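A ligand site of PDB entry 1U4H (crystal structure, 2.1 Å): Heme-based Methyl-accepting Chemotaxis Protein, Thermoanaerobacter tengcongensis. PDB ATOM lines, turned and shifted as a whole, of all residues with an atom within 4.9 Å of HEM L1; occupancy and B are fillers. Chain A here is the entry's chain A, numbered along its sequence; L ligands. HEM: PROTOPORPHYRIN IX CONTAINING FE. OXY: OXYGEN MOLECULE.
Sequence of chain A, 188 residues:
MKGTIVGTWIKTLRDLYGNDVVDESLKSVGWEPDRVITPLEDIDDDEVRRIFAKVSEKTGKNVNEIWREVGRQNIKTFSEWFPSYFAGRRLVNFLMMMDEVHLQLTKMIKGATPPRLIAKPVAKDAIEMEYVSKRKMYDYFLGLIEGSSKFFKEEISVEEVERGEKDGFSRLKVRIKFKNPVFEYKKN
SD of Met 1 sits close to O2A of HEM L1.
An oxygen (O1A) of HEM L1 sits close to the backbone carbonyl oxygen of Thr 113.
Residues that only touch HEM L1: Ile 5, Phe 78, Tyr 85, Phe 86, Phe 94, Met 98, Leu 105, Thr 106, Pro 114, Pro 115, Leu 117, Met 129, Met 137, Tyr 140, Phe 141, Leu 144 and Ser 148.
Hydrophobic or aromatic side chains that line HEM L1: Met 1, Ile 5, Phe 78, Tyr 85, Phe 86, Phe 94, Met 98, His 102, Leu 105, Pro 115, Leu 117, Met 129, Tyr 131, Met 137, Tyr 140, Phe 141 and Leu 144.
Of the 30 residues printed, 24 come within 4 Å of HEM L1.
NE2 of His 102 is bound to FE of HEM L1 (2.1 Å).
O1D of HEM L1 sits at hydrogen-bond distance from OH of Tyr 131.
The side-chain hydroxyl (OG) of Ser 133 is in hydrogen-bond range of an oxygen (O2D) of HEM L1, at 2.7 Å.
O2D of HEM L1 lies within salt-bridge range of NH1 of Arg 135 (2.8 Å).
An oxygen (O2A) of HEM L1 lies within hydrogen-bond range of the backbone NH of Lys 2, 3.0 Å away.
The side-chain hydroxyl (OH) of Tyr 140 is in hydrogen-bond range of an oxygen (O2) of OXY L2 (2.6 Å).
An iron atom (FE) of HEM L1 is bound by an oxygen (O1) of OXY L2 (1.9 Å).
A ring nitrogen (ND1) of His 102 lies within hydrogen-bond range of the backbone carbonyl oxygen of Met 98 (2.6 Å).
OG1 of Thr 106 is in hydrogen-bond range of O of His 102 (2.7 Å).
OH of Tyr 131 sits close to OG of Ser 133, at 3.5 Å.
The side-chain hydroxyl of Tyr 131 lies within hydrogen-bond range of the backbone NH of Met 137, at 2.9 Å.
The side-chain hydroxyl (OG) of Ser 133 lies within hydrogen-bond range of the backbone NH (N) of Arg 135 (3.1 Å).
The guanidinium group of Arg 135 sits at hydrogen-bond distance from the backbone carbonyl oxygen of Thr 113, at 3.1 Å.
O of Leu 144 is in hydrogen-bond range of OG of Ser 148.
OH of Tyr 140 sits at hydrogen-bond distance from NE1 of Trp 9.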
ATOM      1  N   MET A   1      -8.535 -22.586 -19.278  1.00  0.00           N
ATOM      2  CA  MET A   1      -9.730 -22.005 -19.947  1.00  0.00           C
ATOM      3  C   MET A   1      -9.312 -21.248 -21.206  1.00  0.00           C
ATOM      4  O   MET A   1      -8.258 -20.621 -21.248  1.00  0.00           O
ATOM      5  CB  MET A   1     -10.444 -21.041 -18.990  1.00  0.00           C
ATOM      6  CG  MET A   1     -11.917 -20.859 -19.300  1.00  0.00           C
ATOM      7  SD  MET A   1     -12.881 -22.559 -19.137  1.00  0.00           S
ATOM      8  CE  MET A   1     -12.888 -22.662 -17.226  1.00  0.00           C
ATOM      9  N   LYS A   2     -10.151 -21.296 -22.239  1.00  0.00           N
ATOM     10  CA  LYS A   2      -9.834 -20.606 -23.484  1.00  0.00           C
ATOM     11  C   LYS A   2      -9.875 -19.087 -23.247  1.00  0.00           C
ATOM     12  O   LYS A   2     -10.823 -18.550 -22.663  1.00  0.00           O
ATOM     13  CB  LYS A   2     -10.829 -21.002 -24.579  1.00  0.00           C
ATOM     14  CG  LYS A   2     -10.407 -20.568 -25.972  1.00  0.00           C
ATOM     15  CD  LYS A   2     -11.428 -20.976 -27.003  1.00  0.00           C
ATOM     16  CE  LYS A   2     -11.021 -20.470 -28.388  1.00  0.00           C
ATOM     17  NZ  LYS A   2     -12.106 -20.625 -29.380  1.00  0.00           N
ATOM     18  N   ILE A   5     -13.072 -16.856 -23.745  1.00  0.00           N
ATOM     19  CA  ILE A   5     -14.085 -16.971 -22.721  1.00  0.00           C
ATOM     20  C   ILE A   5     -13.717 -16.243 -21.433  1.00  0.00           C
ATOM     21  O   ILE A   5     -14.569 -15.605 -20.808  1.00  0.00           O
ATOM     22  CB  ILE A   5     -14.364 -18.459 -22.433  1.00  0.00           C
ATOM     23  CG1 ILE A   5     -14.834 -19.116 -23.739  1.00  0.00           C
ATOM     24  CG2 ILE A   5     -15.417 -18.626 -21.352  1.00  0.00           C
ATOM     25  CD1 ILE A   5     -15.953 -18.369 -24.432  1.00  0.00           C
ATOM     26  N   TRP A   9     -15.698 -13.279 -19.394  1.00  0.00           N
ATOM     27  CA  TRP A   9     -15.953 -13.292 -17.966  1.00  0.00           C
ATOM     28  C   TRP A   9     -15.514 -12.001 -17.285  1.00  0.00           C
ATOM     29  O   TRP A   9     -16.190 -11.497 -16.405  1.00  0.00           O
ATOM     30  CB  TRP A   9     -15.258 -14.475 -17.285  1.00  0.00           C
ATOM     31  CG  TRP A   9     -15.853 -15.794 -17.643  1.00  0.00           C
ATOM     32  CD1 TRP A   9     -17.067 -16.027 -18.261  1.00  0.00           C
ATOM     33  CD2 TRP A   9     -15.275 -17.082 -17.413  1.00  0.00           C
ATOM     34  NE1 TRP A   9     -17.265 -17.377 -18.427  1.00  0.00           N
ATOM     35  CE2 TRP A   9     -16.172 -18.046 -17.923  1.00  0.00           C
ATOM     36  CE3 TRP A   9     -14.076 -17.503 -16.835  1.00  0.00           C
ATOM     37  CZ2 TRP A   9     -15.920 -19.418 -17.860  1.00  0.00           C
ATOM     38  CZ3 TRP A   9     -13.815 -18.876 -16.768  1.00  0.00           C
ATOM     39  CH2 TRP A   9     -14.735 -19.806 -17.288  1.00  0.00           C
ATOM     40  N   ILE A  75     -24.592 -14.838 -20.785  1.00  0.00           N
ATOM     41  CA  ILE A  75     -25.384 -15.155 -21.961  1.00  0.00           C
ATOM     42  C   ILE A  75     -25.604 -13.858 -22.743  1.00  0.00           C
ATOM     43  O   ILE A  75     -25.563 -13.837 -23.973  1.00  0.00           O
ATOM     44  CB  ILE A  75     -26.760 -15.773 -21.573  1.00  0.00           C
ATOM     45  CG1 ILE A  75     -26.568 -17.210 -21.056  1.00  0.00           C
ATOM     46  CG2 ILE A  75     -27.725 -15.764 -22.765  1.00  0.00           C
ATOM     47  CD1 ILE A  75     -26.000 -18.178 -22.088  1.00  0.00           C
ATOM     48  N   PHE A  78     -22.495 -12.922 -24.362  1.00  0.00           N
ATOM     49  CA  PHE A  78     -22.335 -13.840 -25.492  1.00  0.00           C
ATOM     50  C   PHE A  78     -23.143 -13.400 -26.707  1.00  0.00           C
ATOM     51  O   PHE A  78     -22.669 -13.485 -27.836  1.00  0.00           O
ATOM     52  CB  PHE A  78     -22.769 -15.254 -25.107  1.00  0.00           C
ATOM     53  CG  PHE A  78     -21.679 -16.092 -24.515  1.00  0.00           C
ATOM     54  CD1 PHE A  78     -21.977 -17.086 -23.584  1.00  0.00           C
ATOM     55  CD2 PHE A  78     -20.345 -15.928 -24.907  1.00  0.00           C
ATOM     56  CE1 PHE A  78     -20.977 -17.900 -23.056  1.00  0.00           C
ATOM     57  CE2 PHE A  78     -19.342 -16.730 -24.385  1.00  0.00           C
ATOM     58  CZ  PHE A  78     -19.662 -17.724 -23.452  1.00  0.00           C
ATOM     59  N   PHE A  82     -21.092 -12.995 -29.849  1.00  0.00           N
ATOM     60  CA  PHE A  82     -21.372 -14.080 -30.790  1.00  0.00           C
ATOM     61  C   PHE A  82     -22.846 -14.077 -31.196  1.00  0.00           C
ATOM     62  O   PHE A  82     -23.544 -15.087 -31.045  1.00  0.00           O
ATOM     63  CB  PHE A  82     -21.055 -15.445 -30.149  1.00  0.00           C
ATOM     64  CG  PHE A  82     -19.661 -15.572 -29.603  1.00  0.00           C
ATOM     65  CD1 PHE A  82     -19.264 -14.811 -28.497  1.00  0.00           C
ATOM     66  CD2 PHE A  82     -18.751 -16.466 -30.167  1.00  0.00           C
ATOM     67  CE1 PHE A  82     -17.974 -14.942 -27.962  1.00  0.00           C
ATOM     68  CE2 PHE A  82     -17.461 -16.606 -29.635  1.00  0.00           C
ATOM     69  CZ  PHE A  82     -17.073 -15.845 -28.533  1.00  0.00           C
ATOM     70  N   TYR A  85     -24.964 -17.089 -32.982  1.00  0.00           N
ATOM     71  CA  TYR A  85     -25.484 -18.294 -32.344  1.00  0.00           C
ATOM     72  C   TYR A  85     -26.910 -18.155 -31.817  1.00  0.00           C
ATOM     73  O   TYR A  85     -27.621 -19.138 -31.650  1.00  0.00           O
ATOM     74  CB  TYR A  85     -24.569 -18.736 -31.187  1.00  0.00           C
ATOM     75  CG  TYR A  85     -23.333 -19.473 -31.638  1.00  0.00           C
ATOM     76  CD1 TYR A  85     -22.100 -18.833 -31.691  1.00  0.00           C
ATOM     77  CD2 TYR A  85     -23.420 -20.805 -32.036  1.00  0.00           C
ATOM     78  CE1 TYR A  85     -20.954 -19.517 -32.139  1.00  0.00           C
ATOM     79  CE2 TYR A  85     -22.287 -21.490 -32.479  1.00  0.00           C
ATOM     80  CZ  TYR A  85     -21.064 -20.840 -32.532  1.00  0.00           C
ATOM     81  OH  TYR A  85     -19.963 -21.534 -32.980  1.00  0.00           O
ATOM     82  N   PHE A  86     -27.328 -16.910 -31.572  1.00  0.00           N
ATOM     83  CA  PHE A  86     -28.654 -16.640 -31.059  1.00  0.00           C
ATOM     84  C   PHE A  86     -29.627 -16.246 -32.167  1.00  0.00           C
ATOM     85  O   PHE A  86     -30.834 -16.455 -32.044  1.00  0.00           O
ATOM     86  CB  PHE A  86     -28.569 -15.523 -30.019  1.00  0.00           C
ATOM     87  CG  PHE A  86     -27.636 -15.829 -28.886  1.00  0.00           C
ATOM     88  CD1 PHE A  86     -28.104 -16.427 -27.718  1.00  0.00           C
ATOM     89  CD2 PHE A  86     -26.268 -15.578 -29.017  1.00  0.00           C
ATOM     90  CE1 PHE A  86     -27.229 -16.756 -26.698  1.00  0.00           C
ATOM     91  CE2 PHE A  86     -25.388 -15.911 -27.985  1.00  0.00           C
ATOM     92  CZ  PHE A  86     -25.871 -16.503 -26.833  1.00  0.00           C
ATOM     93  N   PHE A  94     -31.211 -23.934 -29.115  1.00  0.00           N
ATOM     94  CA  PHE A  94     -29.969 -23.391 -28.594  1.00  0.00           C
ATOM     95  C   PHE A  94     -29.246 -24.408 -27.695  1.00  0.00           C
ATOM     96  O   PHE A  94     -28.063 -24.713 -27.893  1.00  0.00           O
ATOM     97  CB  PHE A  94     -30.266 -22.120 -27.798  1.00  0.00           C
ATOM     98  CG  PHE A  94     -29.038 -21.422 -27.297  1.00  0.00           C
ATOM     99  CD1 PHE A  94     -28.220 -20.709 -28.174  1.00  0.00           C
ATOM    100  CD2 PHE A  94     -28.701 -21.480 -25.943  1.00  0.00           C
ATOM    101  CE1 PHE A  94     -27.083 -20.052 -27.703  1.00  0.00           C
ATOM    102  CE2 PHE A  94     -27.555 -20.824 -25.469  1.00  0.00           C
ATOM    103  CZ  PHE A  94     -26.746 -20.110 -26.349  1.00  0.00           C
ATOM    104  N   LEU A  95     -29.969 -24.945 -26.717  1.00  0.00           N
ATOM    105  CA  LEU A  95     -29.404 -25.902 -25.773  1.00  0.00           C
ATOM    106  C   LEU A  95     -28.931 -27.225 -26.398  1.00  0.00           C
ATOM    107  O   LEU A  95     -27.886 -27.742 -26.021  1.00  0.00           O
ATOM    108  CB  LEU A  95     -30.411 -26.178 -24.654  1.00  0.00           C
ATOM    109  CG  LEU A  95     -30.803 -24.950 -23.822  1.00  0.00           C
ATOM    110  CD1 LEU A  95     -31.992 -25.301 -22.908  1.00  0.00           C
ATOM    111  CD2 LEU A  95     -29.604 -24.468 -23.009  1.00  0.00           C
ATOM    112  N   MET A  98     -25.431 -26.773 -27.951  1.00  0.00           N
ATOM    113  CA  MET A  98     -24.259 -26.508 -27.123  1.00  0.00           C
ATOM    114  C   MET A  98     -23.098 -27.516 -27.073  1.00  0.00           C
ATOM    115  O   MET A  98     -21.943 -27.109 -27.126  1.00  0.00           O
ATOM    116  CB  MET A  98     -24.704 -26.155 -25.706  1.00  0.00           C
ATOM    117  CG  MET A  98     -25.424 -24.807 -25.622  1.00  0.00           C
ATOM    118  SD  MET A  98     -24.359 -23.334 -26.346  1.00  0.00           S
ATOM    119  CE  MET A  98     -24.959 -23.376 -28.188  1.00  0.00           C
ATOM    120  N   VAL A 101     -21.245 -27.112 -30.264  1.00  0.00           N
ATOM    121  CA  VAL A 101     -20.590 -25.793 -30.269  1.00  0.00           C
ATOM    122  C   VAL A 101     -19.292 -25.793 -29.445  1.00  0.00           C
ATOM    123  O   VAL A 101     -18.261 -25.284 -29.903  1.00  0.00           O
ATOM    124  CB  VAL A 101     -21.544 -24.705 -29.713  1.00  0.00           C
ATOM    125  CG1 VAL A 101     -20.780 -23.401 -29.437  1.00  0.00           C
ATOM    126  CG2 VAL A 101     -22.667 -24.447 -30.703  1.00  0.00           C
ATOM    127  N   HIS A 102     -19.346 -26.353 -28.249  1.00  0.00           N
ATOM    128  CA  HIS A 102     -18.158 -26.391 -27.405  1.00  0.00           C
ATOM    129  C   HIS A 102     -17.028 -27.219 -28.013  1.00  0.00           C
ATOM    130  O   HIS A 102     -15.848 -26.918 -27.796  1.00  0.00           O
ATOM    131  CB  HIS A 102     -18.546 -26.871 -26.003  1.00  0.00           C
ATOM    132  CG  HIS A 102     -19.306 -25.855 -25.219  1.00  0.00           C
ATOM    133  ND1 HIS A 102     -20.592 -25.467 -25.549  1.00  0.00           N
ATOM    134  CD2 HIS A 102     -18.918 -25.038 -24.211  1.00  0.00           C
ATOM    135  CE1 HIS A 102     -20.949 -24.452 -24.776  1.00  0.00           C
ATOM    136  NE2 HIS A 102     -19.953 -24.170 -23.960  1.00  0.00           N
ATOM    137  N   LEU A 105     -15.623 -24.985 -31.053  1.00  0.00           N
ATOM    138  CA  LEU A 105     -14.871 -23.838 -30.575  1.00  0.00           C
ATOM    139  C   LEU A 105     -13.583 -24.172 -29.826  1.00  0.00           C
ATOM    140  O   LEU A 105     -12.880 -23.262 -29.394  1.00  0.00           O
ATOM    141  CB  LEU A 105     -15.769 -22.948 -29.699  1.00  0.00           C
ATOM    142  CG  LEU A 105     -16.933 -22.266 -30.446  1.00  0.00           C
ATOM    143  CD1 LEU A 105     -17.699 -21.384 -29.494  1.00  0.00           C
ATOM    144  CD2 LEU A 105     -16.391 -21.458 -31.611  1.00  0.00           C
ATOM    145  N   THR A 106     -13.270 -25.454 -29.661  1.00  0.00           N
ATOM    146  CA  THR A 106     -12.024 -25.843 -28.995  1.00  0.00           C
ATOM    147  C   THR A 106     -11.222 -26.833 -29.854  1.00  0.00           C
ATOM    148  O   THR A 106     -10.105 -27.215 -29.503  1.00  0.00           O
ATOM    149  CB  THR A 106     -12.284 -26.493 -27.597  1.00  0.00           C
ATOM    150  OG1 THR A 106     -13.187 -27.596 -27.714  1.00  0.00           O
ATOM    151  CG2 THR A 106     -12.872 -25.458 -26.631  1.00  0.00           C
ATOM    152  N   THR A 113     -10.051 -29.592 -23.499  1.00  0.00           N
ATOM    153  CA  THR A 113     -10.904 -30.297 -22.554  1.00  0.00           C
ATOM    154  C   THR A 113     -12.194 -29.526 -22.320  1.00  0.00           C
ATOM    155  O   THR A 113     -12.513 -29.132 -21.200  1.00  0.00           O
ATOM    156  CB  THR A 113     -10.214 -30.491 -21.189  1.00  0.00           C
ATOM    157  OG1 THR A 113      -9.871 -29.217 -20.635  1.00  0.00           O
ATOM    158  CG2 THR A 113      -8.952 -31.342 -21.350  1.00  0.00           C
ATOM    159  N   PRO A 114     -12.982 -29.318 -23.390  1.00  0.00           N
ATOM    160  CA  PRO A 114     -14.224 -28.580 -23.181  1.00  0.00           C
ATOM    161  C   PRO A 114     -15.205 -29.386 -22.338  1.00  0.00           C
ATOM    162  O   PRO A 114     -15.066 -30.603 -22.200  1.00  0.00           O
ATOM    163  CB  PRO A 114     -14.731 -28.369 -24.600  1.00  0.00           C
ATOM    164  CG  PRO A 114     -14.274 -29.633 -25.302  1.00  0.00           C
ATOM    165  CD  PRO A 114     -12.851 -29.772 -24.782  1.00  0.00           C
ATOM    166  N   PRO A 115     -16.194 -28.716 -21.737  1.00  0.00           N
ATOM    167  CA  PRO A 115     -17.149 -29.471 -20.944  1.00  0.00           C
ATOM    168  C   PRO A 115     -18.045 -30.190 -21.939  1.00  0.00           C
ATOM    169  O   PRO A 115     -18.239 -29.701 -23.048  1.00  0.00           O
ATOM    170  CB  PRO A 115     -17.904 -28.378 -20.200  1.00  0.00           C
ATOM    171  CG  PRO A 115     -17.925 -27.257 -21.210  1.00  0.00           C
ATOM    172  CD  PRO A 115     -16.505 -27.271 -21.731  1.00  0.00           C
ATOM    173  N   LEU A 117     -21.758 -31.374 -22.898  1.00  0.00           N
ATOM    174  CA  LEU A 117     -23.092 -30.908 -22.548  1.00  0.00           C
ATOM    175  C   LEU A 117     -24.199 -31.627 -23.324  1.00  0.00           C
ATOM    176  O   LEU A 117     -25.179 -31.018 -23.722  1.00  0.00           O
ATOM    177  CB  LEU A 117     -23.170 -29.400 -22.821  1.00  0.00           C
ATOM    178  CG  LEU A 117     -22.070 -28.530 -22.200  1.00  0.00           C
ATOM    179  CD1 LEU A 117     -21.884 -27.249 -23.010  1.00  0.00           C
ATOM    180  CD2 LEU A 117     -22.429 -28.223 -20.774  1.00  0.00           C
ATOM    181  N   MET A 129     -30.240 -32.851 -19.764  1.00  0.00           N
ATOM    182  CA  MET A 129     -28.961 -32.297 -20.147  1.00  0.00           C
ATOM    183  C   MET A 129     -27.947 -32.628 -19.068  1.00  0.00           C
ATOM    184  O   MET A 129     -28.198 -32.399 -17.874  1.00  0.00           O
ATOM    185  CB  MET A 129     -29.097 -30.791 -20.353  1.00  0.00           C
ATOM    186  CG  MET A 129     -27.838 -30.096 -20.832  1.00  0.00           C
ATOM    187  SD  MET A 129     -28.201 -28.267 -21.342  1.00  0.00           S
ATOM    188  CE  MET A 129     -27.023 -28.157 -22.869  1.00  0.00           C
ATOM    189  N   TYR A 131     -24.078 -32.095 -17.711  1.00  0.00           N
ATOM    190  CA  TYR A 131     -22.817 -31.384 -17.728  1.00  0.00           C
ATOM    191  C   TYR A 131     -21.757 -32.399 -17.267  1.00  0.00           C
ATOM    192  O   TYR A 131     -21.913 -33.057 -16.239  1.00  0.00           O
ATOM    193  CB  TYR A 131     -22.883 -30.222 -16.724  1.00  0.00           C
ATOM    194  CG  TYR A 131     -21.547 -29.619 -16.347  1.00  0.00           C
ATOM    195  CD1 TYR A 131     -20.858 -28.774 -17.232  1.00  0.00           C
ATOM    196  CD2 TYR A 131     -20.961 -29.903 -15.114  1.00  0.00           C
ATOM    197  CE1 TYR A 131     -19.617 -28.224 -16.880  1.00  0.00           C
ATOM    198  CE2 TYR A 131     -19.724 -29.356 -14.753  1.00  0.00           C
ATOM    199  CZ  TYR A 131     -19.066 -28.511 -15.640  1.00  0.00           C
ATOM    200  OH  TYR A 131     -17.849 -27.982 -15.260  1.00  0.00           O
ATOM    201  N   SER A 133     -17.534 -32.571 -16.872  1.00  0.00           N
ATOM    202  CA  SER A 133     -16.271 -31.850 -16.975  1.00  0.00           C
ATOM    203  C   SER A 133     -15.455 -32.031 -15.712  1.00  0.00           C
ATOM    204  O   SER A 133     -15.987 -32.275 -14.642  1.00  0.00           O
ATOM    205  CB  SER A 133     -16.552 -30.365 -17.205  1.00  0.00           C
ATOM    206  OG  SER A 133     -15.388 -29.587 -17.079  1.00  0.00           O
ATOM    207  N   ARG A 135     -13.729 -29.610 -14.491  1.00  0.00           N
ATOM    208  CA  ARG A 135     -13.669 -28.307 -13.830  1.00  0.00           C
ATOM    209  C   ARG A 135     -14.662 -28.024 -12.704  1.00  0.00           C
ATOM    210  O   ARG A 135     -14.472 -27.082 -11.954  1.00  0.00           O
ATOM    211  CB  ARG A 135     -13.755 -27.186 -14.868  1.00  0.00           C
ATOM    212  CG  ARG A 135     -12.632 -27.199 -15.890  1.00  0.00           C
ATOM    213  CD  ARG A 135     -12.600 -25.900 -16.656  1.00  0.00           C
ATOM    214  NE  ARG A 135     -11.573 -25.903 -17.705  1.00  0.00           N
ATOM    215  CZ  ARG A 135     -11.781 -26.309 -18.950  1.00  0.00           C
ATOM    216  NH1 ARG A 135     -12.980 -26.758 -19.317  1.00  0.00           N
ATOM    217  NH2 ARG A 135     -10.800 -26.265 -19.830  1.00  0.00           N
ATOM    218  N   MET A 137     -17.788 -26.736 -12.634  1.00  0.00           N
ATOM    219  CA  MET A 137     -18.397 -25.406 -12.623  1.00  0.00           C
ATOM    220  C   MET A 137     -19.916 -25.511 -12.721  1.00  0.00           C
ATOM    221  O   MET A 137     -20.552 -24.997 -13.644  1.00  0.00           O
ATOM    222  CB  MET A 137     -17.799 -24.568 -13.754  1.00  0.00           C
ATOM    223  CG  MET A 137     -16.288 -24.329 -13.555  1.00  0.00           C
ATOM    224  SD  MET A 137     -15.344 -23.470 -15.000  1.00  0.00           S
ATOM    225  CE  MET A 137     -13.864 -22.719 -13.998  1.00  0.00           C
ATOM    226  N   TYR A 140     -21.929 -22.145 -12.631  1.00  0.00           N
ATOM    227  CA  TYR A 140     -21.794 -21.423 -13.896  1.00  0.00           C
ATOM    228  C   TYR A 140     -22.771 -22.091 -14.885  1.00  0.00           C
ATOM    229  O   TYR A 140     -23.575 -21.409 -15.524  1.00  0.00           O
ATOM    230  CB  TYR A 140     -20.354 -21.523 -14.416  1.00  0.00           C
ATOM    231  CG  TYR A 140     -20.118 -20.791 -15.715  1.00  0.00           C
ATOM    232  CD1 TYR A 140     -20.475 -19.444 -15.853  1.00  0.00           C
ATOM    233  CD2 TYR A 140     -19.553 -21.447 -16.821  1.00  0.00           C
ATOM    234  CE1 TYR A 140     -20.275 -18.778 -17.054  1.00  0.00           C
ATOM    235  CE2 TYR A 140     -19.353 -20.782 -18.022  1.00  0.00           C
ATOM    236  CZ  TYR A 140     -19.711 -19.454 -18.134  1.00  0.00           C
ATOM    237  OH  TYR A 140     -19.515 -18.782 -19.322  1.00  0.00           O
ATOM    238  N   PHE A 141     -22.695 -23.411 -14.993  1.00  0.00           N
ATOM    239  CA  PHE A 141     -23.567 -24.192 -15.873  1.00  0.00           C
ATOM    240  C   PHE A 141     -25.045 -23.904 -15.613  1.00  0.00           C
ATOM    241  O   PHE A 141     -25.800 -23.639 -16.547  1.00  0.00           O
ATOM    242  CB  PHE A 141     -23.262 -25.685 -15.682  1.00  0.00           C
ATOM    243  CG  PHE A 141     -24.267 -26.603 -16.348  1.00  0.00           C
ATOM    244  CD1 PHE A 141     -24.276 -26.749 -17.736  1.00  0.00           C
ATOM    245  CD2 PHE A 141     -25.166 -27.340 -15.582  1.00  0.00           C
ATOM    246  CE1 PHE A 141     -25.193 -27.620 -18.360  1.00  0.00           C
ATOM    247  CE2 PHE A 141     -26.080 -28.209 -16.181  1.00  0.00           C
ATOM    248  CZ  PHE A 141     -26.095 -28.360 -17.585  1.00  0.00           C
ATOM    249  N   LEU A 144     -25.965 -20.299 -16.687  1.00  0.00           N
ATOM    250  CA  LEU A 144     -26.068 -20.118 -18.127  1.00  0.00           C
ATOM    251  C   LEU A 144     -27.422 -20.589 -18.637  1.00  0.00           C
ATOM    252  O   LEU A 144     -28.009 -19.976 -19.539  1.00  0.00           O
ATOM    253  CB  LEU A 144     -24.953 -20.886 -18.845  1.00  0.00           C
ATOM    254  CG  LEU A 144     -23.529 -20.323 -18.719  1.00  0.00           C
ATOM    255  CD1 LEU A 144     -22.495 -21.361 -19.121  1.00  0.00           C
ATOM    256  CD2 LEU A 144     -23.393 -19.086 -19.554  1.00  0.00           C
ATOM    257  N   ILE A 145     -27.926 -21.670 -18.051  1.00  0.00           N
ATOM    258  CA  ILE A 145     -29.224 -22.203 -18.445  1.00  0.00           C
ATOM    259  C   ILE A 145     -30.288 -21.182 -18.085  1.00  0.00           C
ATOM    260  O   ILE A 145     -31.125 -20.837 -18.912  1.00  0.00           O
ATOM    261  CB  ILE A 145     -29.527 -23.538 -17.749  1.00  0.00           C
ATOM    262  CG1 ILE A 145     -28.575 -24.611 -18.289  1.00  0.00           C
ATOM    263  CG2 ILE A 145     -30.982 -23.953 -17.963  1.00  0.00           C
ATOM    264  CD1 ILE A 145     -28.663 -25.930 -17.554  1.00  0.00           C
ATOM    265  N   SER A 148     -30.096 -18.233 -20.284  1.00  0.00           N
ATOM    266  CA  SER A 148     -30.569 -18.569 -21.628  1.00  0.00           C
ATOM    267  C   SER A 148     -32.090 -18.498 -21.654  1.00  0.00           C
ATOM    268  O   SER A 148     -32.681 -18.047 -22.638  1.00  0.00           O
ATOM    269  CB  SER A 148     -30.112 -19.976 -22.015  1.00  0.00           C
ATOM    270  OG  SER A 148     -28.709 -20.046 -22.106  1.00  0.00           O
HETATM  271  CHA HEM L   1     -16.919 -23.069 -21.242  1.00  0.00           C
HETATM  272  CHB HEM L   1     -18.313 -21.207 -25.530  1.00  0.00           C
HETATM  273  CHC HEM L   1     -22.888 -21.161 -23.905  1.00  0.00           C
HETATM  274  CHD HEM L   1     -21.511 -24.395 -20.536  1.00  0.00           C
HETATM  275  C1A HEM L   1     -16.889 -22.586 -22.578  1.00  0.00           C
HETATM  276  C2A HEM L   1     -15.702 -22.552 -23.409  1.00  0.00           C
HETATM  277  C3A HEM L   1     -16.132 -22.097 -24.619  1.00  0.00           C
HETATM  278  C4A HEM L   1     -17.547 -21.796 -24.521  1.00  0.00           C
HETATM  279  CMA HEM L   1     -15.245 -21.887 -25.846  1.00  0.00           C
HETATM  280  CAA HEM L   1     -14.242 -22.856 -23.022  1.00  0.00           C
HETATM  281  CBA HEM L   1     -13.984 -24.354 -23.023  1.00  0.00           C
HETATM  282  CGA HEM L   1     -12.552 -24.718 -22.645  1.00  0.00           C
HETATM  283  O1A HEM L   1     -12.294 -25.935 -22.481  1.00  0.00           O
HETATM  284  O2A HEM L   1     -11.694 -23.820 -22.517  1.00  0.00           O
HETATM  285  C1B HEM L   1     -19.679 -20.966 -25.443  1.00  0.00           C
HETATM  286  C2B HEM L   1     -20.447 -20.155 -26.388  1.00  0.00           C
HETATM  287  C3B HEM L   1     -21.732 -20.091 -25.894  1.00  0.00           C
HETATM  288  C4B HEM L   1     -21.753 -20.920 -24.687  1.00  0.00           C
HETATM  289  CMB HEM L   1     -19.888 -19.490 -27.630  1.00  0.00           C
HETATM  290  CAB HEM L   1     -22.789 -19.316 -26.369  1.00  0.00           C
HETATM  291  CBB HEM L   1     -23.289 -19.424 -27.725  1.00  0.00           C
HETATM  292  C1C HEM L   1     -22.944 -22.171 -22.935  1.00  0.00           C
HETATM  293  C2C HEM L   1     -24.165 -22.776 -22.408  1.00  0.00           C
HETATM  294  C3C HEM L   1     -23.753 -23.742 -21.521  1.00  0.00           C
HETATM  295  C4C HEM L   1     -22.310 -23.730 -21.487  1.00  0.00           C
HETATM  296  CMC HEM L   1     -25.619 -22.355 -22.707  1.00  0.00           C
HETATM  297  CAC HEM L   1     -24.555 -24.517 -20.682  1.00  0.00           C
HETATM  298  CBC HEM L   1     -25.689 -25.282 -21.086  1.00  0.00           C
HETATM  299  C1D HEM L   1     -20.184 -24.051 -20.264  1.00  0.00           C
HETATM  300  C2D HEM L   1     -19.459 -24.347 -19.034  1.00  0.00           C
HETATM  301  C3D HEM L   1     -18.176 -23.973 -19.238  1.00  0.00           C
HETATM  302  C4D HEM L   1     -18.090 -23.481 -20.604  1.00  0.00           C
HETATM  303  CMD HEM L   1     -20.026 -24.990 -17.764  1.00  0.00           C
HETATM  304  CAD HEM L   1     -17.050 -23.866 -18.199  1.00  0.00           C
HETATM  305  CBD HEM L   1     -15.879 -24.830 -18.335  1.00  0.00           C
HETATM  306  CGD HEM L   1     -16.190 -26.212 -17.807  1.00  0.00           C
HETATM  307  O1D HEM L   1     -17.141 -26.352 -17.016  1.00  0.00           O
HETATM  308  O2D HEM L   1     -15.459 -27.154 -18.168  1.00  0.00           O
HETATM  309  NA  HEM L   1     -18.040 -22.135 -23.274  1.00  0.00           N
HETATM  310  NB  HEM L   1     -20.482 -21.441 -24.398  1.00  0.00           N
HETATM  311  NC  HEM L   1     -21.810 -22.768 -22.366  1.00  0.00           N
HETATM  312  ND  HEM L   1     -19.351 -23.485 -21.208  1.00  0.00           N
HETATM  313 FE   HEM L   1     -19.917 -22.389 -22.789  1.00  0.00          FE
HETATM  314  O1  OXY L   2     -19.979 -20.831 -21.760  1.00  0.00           O
HETATM  315  O2  OXY L   2     -18.889 -20.188 -21.428  1.00  0.00           O
